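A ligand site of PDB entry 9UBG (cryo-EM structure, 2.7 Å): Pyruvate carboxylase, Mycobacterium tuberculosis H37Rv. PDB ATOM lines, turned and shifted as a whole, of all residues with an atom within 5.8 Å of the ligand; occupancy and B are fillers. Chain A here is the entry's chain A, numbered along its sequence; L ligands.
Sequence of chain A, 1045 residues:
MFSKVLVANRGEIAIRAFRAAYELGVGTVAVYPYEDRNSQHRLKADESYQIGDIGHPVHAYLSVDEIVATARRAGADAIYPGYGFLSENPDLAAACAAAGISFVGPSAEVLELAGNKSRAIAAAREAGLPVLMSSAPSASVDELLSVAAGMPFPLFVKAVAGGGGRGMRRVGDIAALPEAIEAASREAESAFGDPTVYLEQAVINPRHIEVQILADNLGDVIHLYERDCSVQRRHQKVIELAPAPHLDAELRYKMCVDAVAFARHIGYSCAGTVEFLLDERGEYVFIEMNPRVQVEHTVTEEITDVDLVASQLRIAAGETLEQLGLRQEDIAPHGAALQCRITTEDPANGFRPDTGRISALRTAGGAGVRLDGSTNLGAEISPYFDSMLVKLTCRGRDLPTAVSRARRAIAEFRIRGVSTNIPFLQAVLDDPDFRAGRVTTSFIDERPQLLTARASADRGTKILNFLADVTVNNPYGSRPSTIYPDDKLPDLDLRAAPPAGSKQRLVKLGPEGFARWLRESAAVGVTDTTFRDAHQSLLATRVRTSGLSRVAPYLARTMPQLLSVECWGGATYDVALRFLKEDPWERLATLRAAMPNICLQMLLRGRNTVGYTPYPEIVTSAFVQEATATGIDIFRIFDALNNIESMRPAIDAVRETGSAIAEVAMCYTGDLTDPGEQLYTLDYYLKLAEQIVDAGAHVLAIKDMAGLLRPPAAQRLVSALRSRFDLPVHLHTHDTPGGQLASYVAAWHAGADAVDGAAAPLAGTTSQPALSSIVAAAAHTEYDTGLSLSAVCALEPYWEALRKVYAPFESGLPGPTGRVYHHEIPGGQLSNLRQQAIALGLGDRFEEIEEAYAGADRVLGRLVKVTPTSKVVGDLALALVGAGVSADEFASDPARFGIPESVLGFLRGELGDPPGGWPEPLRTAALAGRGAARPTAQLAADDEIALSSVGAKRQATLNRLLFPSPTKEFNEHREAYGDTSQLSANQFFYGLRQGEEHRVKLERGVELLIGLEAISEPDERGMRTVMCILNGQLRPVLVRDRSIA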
ATOM      1  N   LYS A 117      30.857  21.410  22.073  1.00  0.00           N
ATOM      2  CA  LYS A 117      29.489  21.909  21.922  1.00  0.00           C
ATOM      3  C   LYS A 117      28.432  21.011  22.557  1.00  0.00           C
ATOM      4  O   LYS A 117      28.642  19.805  22.736  1.00  0.00           O
ATOM      5  CB  LYS A 117      29.150  22.154  20.456  1.00  0.00           C
ATOM      6  CG  LYS A 117      28.150  23.246  20.216  1.00  0.00           C
ATOM      7  CD  LYS A 117      28.340  23.927  18.884  1.00  0.00           C
ATOM      8  CE  LYS A 117      29.477  24.949  18.960  1.00  0.00           C
ATOM      9  NZ  LYS A 117      29.534  25.693  20.267  1.00  0.00           N
ATOM     10  N   PHE A 156      18.153  23.645  10.007  1.00  0.00           N
ATOM     11  CA  PHE A 156      19.530  23.960   9.686  1.00  0.00           C
ATOM     12  C   PHE A 156      20.409  22.758  10.027  1.00  0.00           C
ATOM     13  O   PHE A 156      20.474  22.351  11.190  1.00  0.00           O
ATOM     14  CB  PHE A 156      20.024  25.195  10.443  1.00  0.00           C
ATOM     15  CG  PHE A 156      19.974  26.462   9.649  1.00  0.00           C
ATOM     16  CD1 PHE A 156      20.947  26.733   8.695  1.00  0.00           C
ATOM     17  CD2 PHE A 156      18.973  27.390   9.854  1.00  0.00           C
ATOM     18  CE1 PHE A 156      20.892  27.889   7.935  1.00  0.00           C
ATOM     19  CE2 PHE A 156      18.926  28.556   9.116  1.00  0.00           C
ATOM     20  CZ  PHE A 156      19.887  28.806   8.165  1.00  0.00           C
ATOM     21  N   LYS A 158      24.059  21.687  10.435  1.00  0.00           N
ATOM     22  CA  LYS A 158      25.277  22.400  10.767  1.00  0.00           C
ATOM     23  C   LYS A 158      26.408  21.423  11.027  1.00  0.00           C
ATOM     24  O   LYS A 158      26.198  20.376  11.650  1.00  0.00           O
ATOM     25  CB  LYS A 158      25.057  23.273  12.009  1.00  0.00           C
ATOM     26  CG  LYS A 158      24.264  24.542  11.776  1.00  0.00           C
ATOM     27  CD  LYS A 158      23.420  24.885  12.998  1.00  0.00           C
ATOM     28  CE  LYS A 158      23.175  26.375  13.109  1.00  0.00           C
ATOM     29  NZ  LYS A 158      22.595  26.726  14.427  1.00  0.00           N
ATOM     30  N   GLY A 162      32.027  23.064  12.891  1.00  0.00           N
ATOM     31  CA  GLY A 162      31.913  24.332  12.190  1.00  0.00           C
ATOM     32  C   GLY A 162      31.701  25.491  13.139  1.00  0.00           C
ATOM     33  O   GLY A 162      30.894  25.429  14.069  1.00  0.00           O
ATOM     34  N   GLY A 163      32.440  26.572  12.905  1.00  0.00           N
ATOM     35  CA  GLY A 163      32.326  27.766  13.723  1.00  0.00           C
ATOM     36  C   GLY A 163      32.596  29.039  12.939  1.00  0.00           C
ATOM     37  O   GLY A 163      33.631  29.153  12.276  1.00  0.00           O
ATOM     38  N   GLY A 164      31.675  29.997  13.021  1.00  0.00           N
ATOM     39  CA  GLY A 164      31.757  31.240  12.278  1.00  0.00           C
ATOM     40  C   GLY A 164      30.693  31.393  11.214  1.00  0.00           C
ATOM     41  O   GLY A 164      30.366  32.524  10.838  1.00  0.00           O
ATOM     42  N   GLY A 165      30.099  30.294  10.754  1.00  0.00           N
ATOM     43  CA  GLY A 165      29.235  30.331   9.591  1.00  0.00           C
ATOM     44  C   GLY A 165      29.814  29.587   8.400  1.00  0.00           C
ATOM     45  O   GLY A 165      29.618  29.996   7.247  1.00  0.00           O
ATOM     46  N   MET A 168      26.880  25.097   6.935  1.00  0.00           N
ATOM     47  CA  MET A 168      25.494  24.829   7.300  1.00  0.00           C
ATOM     48  C   MET A 168      24.580  25.047   6.111  1.00  0.00           C
ATOM     49  O   MET A 168      24.847  25.892   5.239  1.00  0.00           O
ATOM     50  CB  MET A 168      24.996  25.692   8.491  1.00  0.00           C
ATOM     51  CG  MET A 168      25.263  27.206   8.449  1.00  0.00           C
ATOM     52  SD  MET A 168      26.930  27.790   8.135  1.00  0.00           S
ATOM     53  CE  MET A 168      27.766  26.986   9.505  1.00  0.00           C
ATOM     54  N   ARG A 170      20.233  25.187   4.980  1.00  0.00           N
ATOM     55  CA  ARG A 170      18.837  25.278   5.384  1.00  0.00           C
ATOM     56  C   ARG A 170      18.009  24.404   4.437  1.00  0.00           C
ATOM     57  O   ARG A 170      18.043  24.600   3.225  1.00  0.00           O
ATOM     58  CB  ARG A 170      18.332  26.726   5.338  1.00  0.00           C
ATOM     59  CG  ARG A 170      16.916  26.871   5.858  1.00  0.00           C
ATOM     60  CD  ARG A 170      16.296  28.245   5.633  1.00  0.00           C
ATOM     61  NE  ARG A 170      16.931  29.292   6.437  1.00  0.00           N
ATOM     62  CZ  ARG A 170      16.348  29.912   7.453  1.00  0.00           C
ATOM     63  NH1 ARG A 170      15.120  29.614   7.825  1.00  0.00           N
ATOM     64  NH2 ARG A 170      17.012  30.871   8.097  1.00  0.00           N
ATOM     65  N   TYR A 198      24.847  18.042  12.777  1.00  0.00           N
ATOM     66  CA  TYR A 198      23.711  18.058  13.679  1.00  0.00           C
ATOM     67  C   TYR A 198      22.641  19.008  13.141  1.00  0.00           C
ATOM     68  O   TYR A 198      22.964  20.035  12.536  1.00  0.00           O
ATOM     69  CB  TYR A 198      24.127  18.483  15.097  1.00  0.00           C
ATOM     70  CG  TYR A 198      24.405  19.961  15.269  1.00  0.00           C
ATOM     71  CD1 TYR A 198      25.646  20.490  14.944  1.00  0.00           C
ATOM     72  CD2 TYR A 198      23.435  20.818  15.769  1.00  0.00           C
ATOM     73  CE1 TYR A 198      25.902  21.839  15.108  1.00  0.00           C
ATOM     74  CE2 TYR A 198      23.687  22.160  15.928  1.00  0.00           C
ATOM     75  CZ  TYR A 198      24.923  22.667  15.601  1.00  0.00           C
ATOM     76  OH  TYR A 198      25.174  24.010  15.760  1.00  0.00           O
ATOM     77  N   GLU A 200      19.150  21.492  13.619  1.00  0.00           N
ATOM     78  CA  GLU A 200      18.589  22.414  14.597  1.00  0.00           C
ATOM     79  C   GLU A 200      17.388  23.123  13.980  1.00  0.00           C
ATOM     80  O   GLU A 200      17.350  23.376  12.774  1.00  0.00           O
ATOM     81  CB  GLU A 200      19.611  23.443  15.097  1.00  0.00           C
ATOM     82  CG  GLU A 200      19.099  24.294  16.231  1.00  0.00           C
ATOM     83  CD  GLU A 200      19.931  25.558  16.429  1.00  0.00           C
ATOM     84  OE1 GLU A 200      20.918  25.511  17.190  1.00  0.00           O
ATOM     85  OE2 GLU A 200      19.582  26.588  15.814  1.00  0.00           O
ATOM     86  N   GLN A 201      16.406  23.430  14.822  1.00  0.00           N
ATOM     87  CA  GLN A 201      15.237  24.199  14.388  1.00  0.00           C
ATOM     88  C   GLN A 201      15.675  25.561  13.879  1.00  0.00           C
ATOM     89  O   GLN A 201      16.491  26.241  14.506  1.00  0.00           O
ATOM     90  CB  GLN A 201      14.244  24.337  15.537  1.00  0.00           C
ATOM     91  CG  GLN A 201      13.233  25.456  15.355  1.00  0.00           C
ATOM     92  CD  GLN A 201      12.415  25.702  16.599  1.00  0.00           C
ATOM     93  OE1 GLN A 201      12.633  25.075  17.639  1.00  0.00           O
ATOM     94  NE2 GLN A 201      11.450  26.608  16.500  1.00  0.00           N
ATOM     95  N   ALA A 202      15.126  25.973  12.739  1.00  0.00           N
ATOM     96  CA  ALA A 202      15.575  27.182  12.042  1.00  0.00           C
ATOM     97  C   ALA A 202      14.648  28.329  12.384  1.00  0.00           C
ATOM     98  O   ALA A 202      13.532  28.435  11.858  1.00  0.00           O
ATOM     99  CB  ALA A 202      15.624  26.938  10.534  1.00  0.00           C
ATOM    100  N   VAL A 203      15.123  29.207  13.274  1.00  0.00           N
ATOM    101  CA  VAL A 203      14.354  30.345  13.748  1.00  0.00           C
ATOM    102  C   VAL A 203      14.344  31.428  12.671  1.00  0.00           C
ATOM    103  O   VAL A 203      15.366  31.708  12.036  1.00  0.00           O
ATOM    104  CB  VAL A 203      14.932  30.874  15.077  1.00  0.00           C
ATOM    105  CG1 VAL A 203      16.428  31.129  14.952  1.00  0.00           C
ATOM    106  CG2 VAL A 203      14.207  32.129  15.527  1.00  0.00           C
ATOM    107  N   HIS A 208      21.295  38.998  16.157  1.00  0.00           N
ATOM    108  CA  HIS A 208      22.381  38.436  16.956  1.00  0.00           C
ATOM    109  C   HIS A 208      22.798  39.431  18.032  1.00  0.00           C
ATOM    110  O   HIS A 208      23.109  40.587  17.729  1.00  0.00           O
ATOM    111  CB  HIS A 208      23.572  38.072  16.060  1.00  0.00           C
ATOM    112  CG  HIS A 208      24.551  37.141  16.718  1.00  0.00           C
ATOM    113  ND1 HIS A 208      25.708  36.725  16.091  1.00  0.00           N
ATOM    114  CD2 HIS A 208      24.525  36.510  17.911  1.00  0.00           C
ATOM    115  CE1 HIS A 208      26.369  35.902  16.887  1.00  0.00           C
ATOM    116  NE2 HIS A 208      25.666  35.758  18.002  1.00  0.00           N
ATOM    117  N   GLN A 232      25.531  40.653   8.379  1.00  0.00           N
ATOM    118  CA  GLN A 232      26.506  39.639   8.028  1.00  0.00           C
ATOM    119  C   GLN A 232      26.448  39.354   6.530  1.00  0.00           C
ATOM    120  O   GLN A 232      25.397  39.491   5.895  1.00  0.00           O
ATOM    121  CB  GLN A 232      26.295  38.330   8.806  1.00  0.00           C
ATOM    122  CG  GLN A 232      25.905  38.515  10.260  1.00  0.00           C
ATOM    123  CD  GLN A 232      26.079  37.243  11.080  1.00  0.00           C
ATOM    124  OE1 GLN A 232      26.418  36.188  10.547  1.00  0.00           O
ATOM    125  NE2 GLN A 232      25.839  37.348  12.381  1.00  0.00           N
ATOM    126  N   HIS A 235      27.286  34.763   6.424  1.00  0.00           N
ATOM    127  CA  HIS A 235      27.376  34.444   7.845  1.00  0.00           C
ATOM    128  C   HIS A 235      28.640  34.968   8.499  1.00  0.00           C
ATOM    129  O   HIS A 235      28.935  34.600   9.648  1.00  0.00           O
ATOM    130  CB  HIS A 235      27.269  32.926   8.078  1.00  0.00           C
ATOM    131  CG  HIS A 235      25.906  32.371   7.826  1.00  0.00           C
ATOM    132  ND1 HIS A 235      24.889  33.112   7.263  1.00  0.00           N
ATOM    133  CD2 HIS A 235      25.418  31.117   7.975  1.00  0.00           C
ATOM    134  CE1 HIS A 235      23.811  32.361   7.134  1.00  0.00           C
ATOM    135  NE2 HIS A 235      24.114  31.142   7.552  1.00  0.00           N
ATOM    136  N   LYS A 237      30.812  38.205  10.035  1.00  0.00           N
ATOM    137  CA  LYS A 237      30.557  39.513  10.613  1.00  0.00           C
ATOM    138  C   LYS A 237      31.151  40.611   9.732  1.00  0.00           C
ATOM    139  O   LYS A 237      32.272  40.483   9.225  1.00  0.00           O
ATOM    140  CB  LYS A 237      31.154  39.580  12.023  1.00  0.00           C
ATOM    141  CG  LYS A 237      30.279  40.308  13.031  1.00  0.00           C
ATOM    142  CD  LYS A 237      30.487  39.752  14.425  1.00  0.00           C
ATOM    143  CE  LYS A 237      30.230  38.252  14.475  1.00  0.00           C
ATOM    144  NZ  LYS A 237      28.856  37.911  14.005  1.00  0.00           N
ATOM    145  N   GLU A 275      26.334  34.526  23.410  1.00  0.00           N
ATOM    146  CA  GLU A 275      25.617  34.882  22.192  1.00  0.00           C
ATOM    147  C   GLU A 275      24.160  34.466  22.272  1.00  0.00           C
ATOM    148  O   GLU A 275      23.836  33.398  22.811  1.00  0.00           O
ATOM    149  CB  GLU A 275      26.281  34.229  20.977  1.00  0.00           C
ATOM    150  CG  GLU A 275      27.699  34.734  20.719  1.00  0.00           C
ATOM    151  CD  GLU A 275      28.272  34.221  19.412  1.00  0.00           C
ATOM    152  OE1 GLU A 275      27.567  33.482  18.690  1.00  0.00           O
ATOM    153  OE2 GLU A 275      29.437  34.567  19.100  1.00  0.00           O
ATOM    154  N   LEU A 277      20.173  34.755  19.979  1.00  0.00           N
ATOM    155  CA  LEU A 277      19.411  35.101  18.787  1.00  0.00           C
ATOM    156  C   LEU A 277      17.990  35.467  19.181  1.00  0.00           C
ATOM    157  O   LEU A 277      17.348  34.750  19.946  1.00  0.00           O
ATOM    158  CB  LEU A 277      19.406  33.952  17.774  1.00  0.00           C
ATOM    159  CG  LEU A 277      20.480  34.018  16.686  1.00  0.00           C
ATOM    160  CD1 LEU A 277      21.889  33.949  17.248  1.00  0.00           C
ATOM    161  CD2 LEU A 277      20.262  32.932  15.650  1.00  0.00           C
ATOM    162  N   ILE A 287      23.123  30.493  21.661  1.00  0.00           N
ATOM    163  CA  ILE A 287      23.835  29.763  20.616  1.00  0.00           C
ATOM    164  C   ILE A 287      25.129  29.167  21.159  1.00  0.00           C
ATOM    165  O   ILE A 287      25.382  27.966  21.024  1.00  0.00           O
ATOM    166  CB  ILE A 287      24.069  30.674  19.390  1.00  0.00           C
ATOM    167  CG1 ILE A 287      22.891  30.595  18.420  1.00  0.00           C
ATOM    168  CG2 ILE A 287      25.317  30.253  18.642  1.00  0.00           C
ATOM    169  CD1 ILE A 287      21.545  30.925  19.022  1.00  0.00           C
ATOM    170  N   GLU A 288      25.951  29.991  21.806  1.00  0.00           N
ATOM    171  CA  GLU A 288      27.158  29.501  22.478  1.00  0.00           C
ATOM    172  C   GLU A 288      27.760  30.609  23.329  1.00  0.00           C
ATOM    173  O   GLU A 288      27.170  31.682  23.521  1.00  0.00           O
ATOM    174  CB  GLU A 288      28.185  28.938  21.493  1.00  0.00           C
ATOM    175  CG  GLU A 288      28.359  29.745  20.217  1.00  0.00           C
ATOM    176  CD  GLU A 288      29.465  30.764  20.332  1.00  0.00           C
ATOM    177  OE1 GLU A 288      30.152  30.774  21.368  1.00  0.00           O
ATOM    178  OE2 GLU A 288      29.647  31.552  19.380  1.00  0.00           O
ATOM    179  N   ASN A 290      31.659  32.332  23.859  1.00  0.00           N
ATOM    180  CA  ASN A 290      33.054  32.446  23.447  1.00  0.00           C
ATOM    181  C   ASN A 290      33.918  32.798  24.655  1.00  0.00           C
ATOM    182  O   ASN A 290      33.724  33.878  25.233  1.00  0.00           O
ATOM    183  CB  ASN A 290      33.227  33.492  22.360  1.00  0.00           C
ATOM    184  CG  ASN A 290      33.184  32.896  20.965  1.00  0.00           C
ATOM    185  OD1 ASN A 290      32.163  32.364  20.530  1.00  0.00           O
ATOM    186  ND2 ASN A 290      34.304  32.998  20.249  1.00  0.00           N
ATOM    187  N   THR A 441      19.397  39.778  10.165  1.00  0.00           N
ATOM    188  CA  THR A 441      20.357  38.817   9.623  1.00  0.00           C
ATOM    189  C   THR A 441      20.295  38.749   8.099  1.00  0.00           C
ATOM    190  O   THR A 441      21.328  38.600   7.433  1.00  0.00           O
ATOM    191  CB  THR A 441      20.117  37.435  10.236  1.00  0.00           C
ATOM    192  OG1 THR A 441      20.648  37.396  11.561  1.00  0.00           O
ATOM    193  CG2 THR A 441      20.761  36.335   9.402  1.00  0.00           C
HETATM  194  P1  LIG L   1      29.867  32.071  15.771  1.00  0.00           P
HETATM  195  O1  LIG L   1      29.939  32.774  14.445  1.00  0.00           O
HETATM  196  O2  LIG L   1      29.978  33.026  16.926  1.00  0.00           O
HETATM  197  O3  LIG L   1      30.845  30.924  15.879  1.00  0.00           O
HETATM  198  P2  LIG L   1      27.700  30.188  15.099  1.00  0.00           P
HETATM  199  O4  LIG L   1      27.068  29.303  16.119  1.00  0.00           O
HETATM  200  O5  LIG L   1      28.690  29.580  14.166  1.00  0.00           O
HETATM  201  O6  LIG L   1      28.395  31.427  15.846  1.00  0.00           O
HETATM  202  O7  LIG L   1      26.562  30.931  14.256  1.00  0.00           O
HETATM  203  C1  LIG L   1      26.979  31.691  13.102  1.00  0.00           C
HETATM  204  C2  LIG L   1      25.776  32.380  12.499  1.00  0.00           C
HETATM  205  O8  LIG L   1      24.944  31.411  11.814  1.00  0.00           O
HETATM  206  C3  LIG L   1      24.780  33.027  13.465  1.00  0.00           C
HETATM  207  O9  LIG L   1      25.255  34.283  13.930  1.00  0.00           O
HETATM  208  C4  LIG L   1      23.559  33.182  12.557  1.00  0.00           C
HETATM  209  O10 LIG L   1      23.546  34.418  11.889  1.00  0.00           O
HETATM  210  C5  LIG L   1      23.717  32.026  11.552  1.00  0.00           C
HETATM  211  N1  LIG L   1      22.660  31.024  11.626  1.00  0.00           N
HETATM  212  C6  LIG L   1      22.037  30.428  10.559  1.00  0.00           C
HETATM  213  N2  LIG L   1      21.114  29.572  10.896  1.00  0.00           N
HETATM  214  C7  LIG L   1      21.118  29.598  12.281  1.00  0.00           C
HETATM  215  C8  LIG L   1      20.355  28.906  13.234  1.00  0.00           C
HETATM  216  N3  LIG L   1      19.422  28.016  12.924  1.00  0.00           N
HETATM  217  N4  LIG L   1      20.611  29.158  14.537  1.00  0.00           N
HETATM  218  C9  LIG L   1      21.569  30.047  14.844  1.00  0.00           C
HETATM  219  N5  LIG L   1      22.336  30.760  14.035  1.00  0.00           N
HETATM  220  C10 LIG L   1      22.065  30.482  12.748  1.00  0.00           C
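N of Glu 275 lies within hydrogen-bond range of O of Glu 288 (3.0 Å).
N of Ile 287 sits at hydrogen-bond distance from O of Glu 275.
The side-chain carboxylate (OE1) of Glu 275 lies within hydrogen-bond range of a ring nitrogen (NE2) of His 208, 3.0 Å away.
OE1 of Glu 288 sits close to OD1 of Asn 290.
The backbone carbonyl oxygen (O) of Glu 200 is in hydrogen-bond range of the backbone NH (N) of Phe 156 (2.9 Å).
The side-chain carboxylate of Glu 200 is in salt-bridge range of the side-chain amino group of Lys 158 (3.3 Å).
N of Lys 158 lies within hydrogen-bond range of O of Tyr 198 (2.9 Å).
The side-chain amide nitrogen (NE2) of Gln 232 lies close to the side-chain amino group (NZ) of Lys 237 (3.5 Å).
Merely in contact with the ligand: Phe 156 (3.0 Å), Ile 287 (3.2 Å), Leu 277 (3.3 Å), His 235 (3.7 Å), Gly 165 (3.8 Å), Gln 201 (3.8 Å) and Gly 163 (3.9 Å).
Hydrophobic or aromatic side chains that line the ligand: Phe 156, His 208, His 235, Leu 277 and Ile 287.
14 residues have an atom within 4 Å of the ligand: Phe 156, Lys 158, Gly 163, Gly 164, Gly 165, Glu 200, Gln 201, His 208, Gln 232, His 235, Glu 275, Leu 277, Ile 287 and Glu 288.
The side-chain carboxylate (OE2) of Glu 275 lies close to an oxygen (O2) of the ligand.
O2 of the ligand lies close to OE2 of Glu 288 (2.9 Å).
The side-chain carboxylate (OE2) of Glu 200 is in hydrogen-bond range of a nitrogen (N3) of the ligand (3.2 Å).
N of Gly 164 lies within hydrogen-bond range of O3 of the ligand, at 3.1 Å.
NZ of Lys 158 lies within hydrogen-bond range of N4 of the ligand.
A ring nitrogen (ND1) of His 208 sits at hydrogen-bond distance from an oxygen (O9) of the ligand (3.3 Å).
The side-chain amide nitrogen (NE2) of Gln 232 sits at hydrogen-bond distance from an oxygen (O9) of the ligand (3.5 Å).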
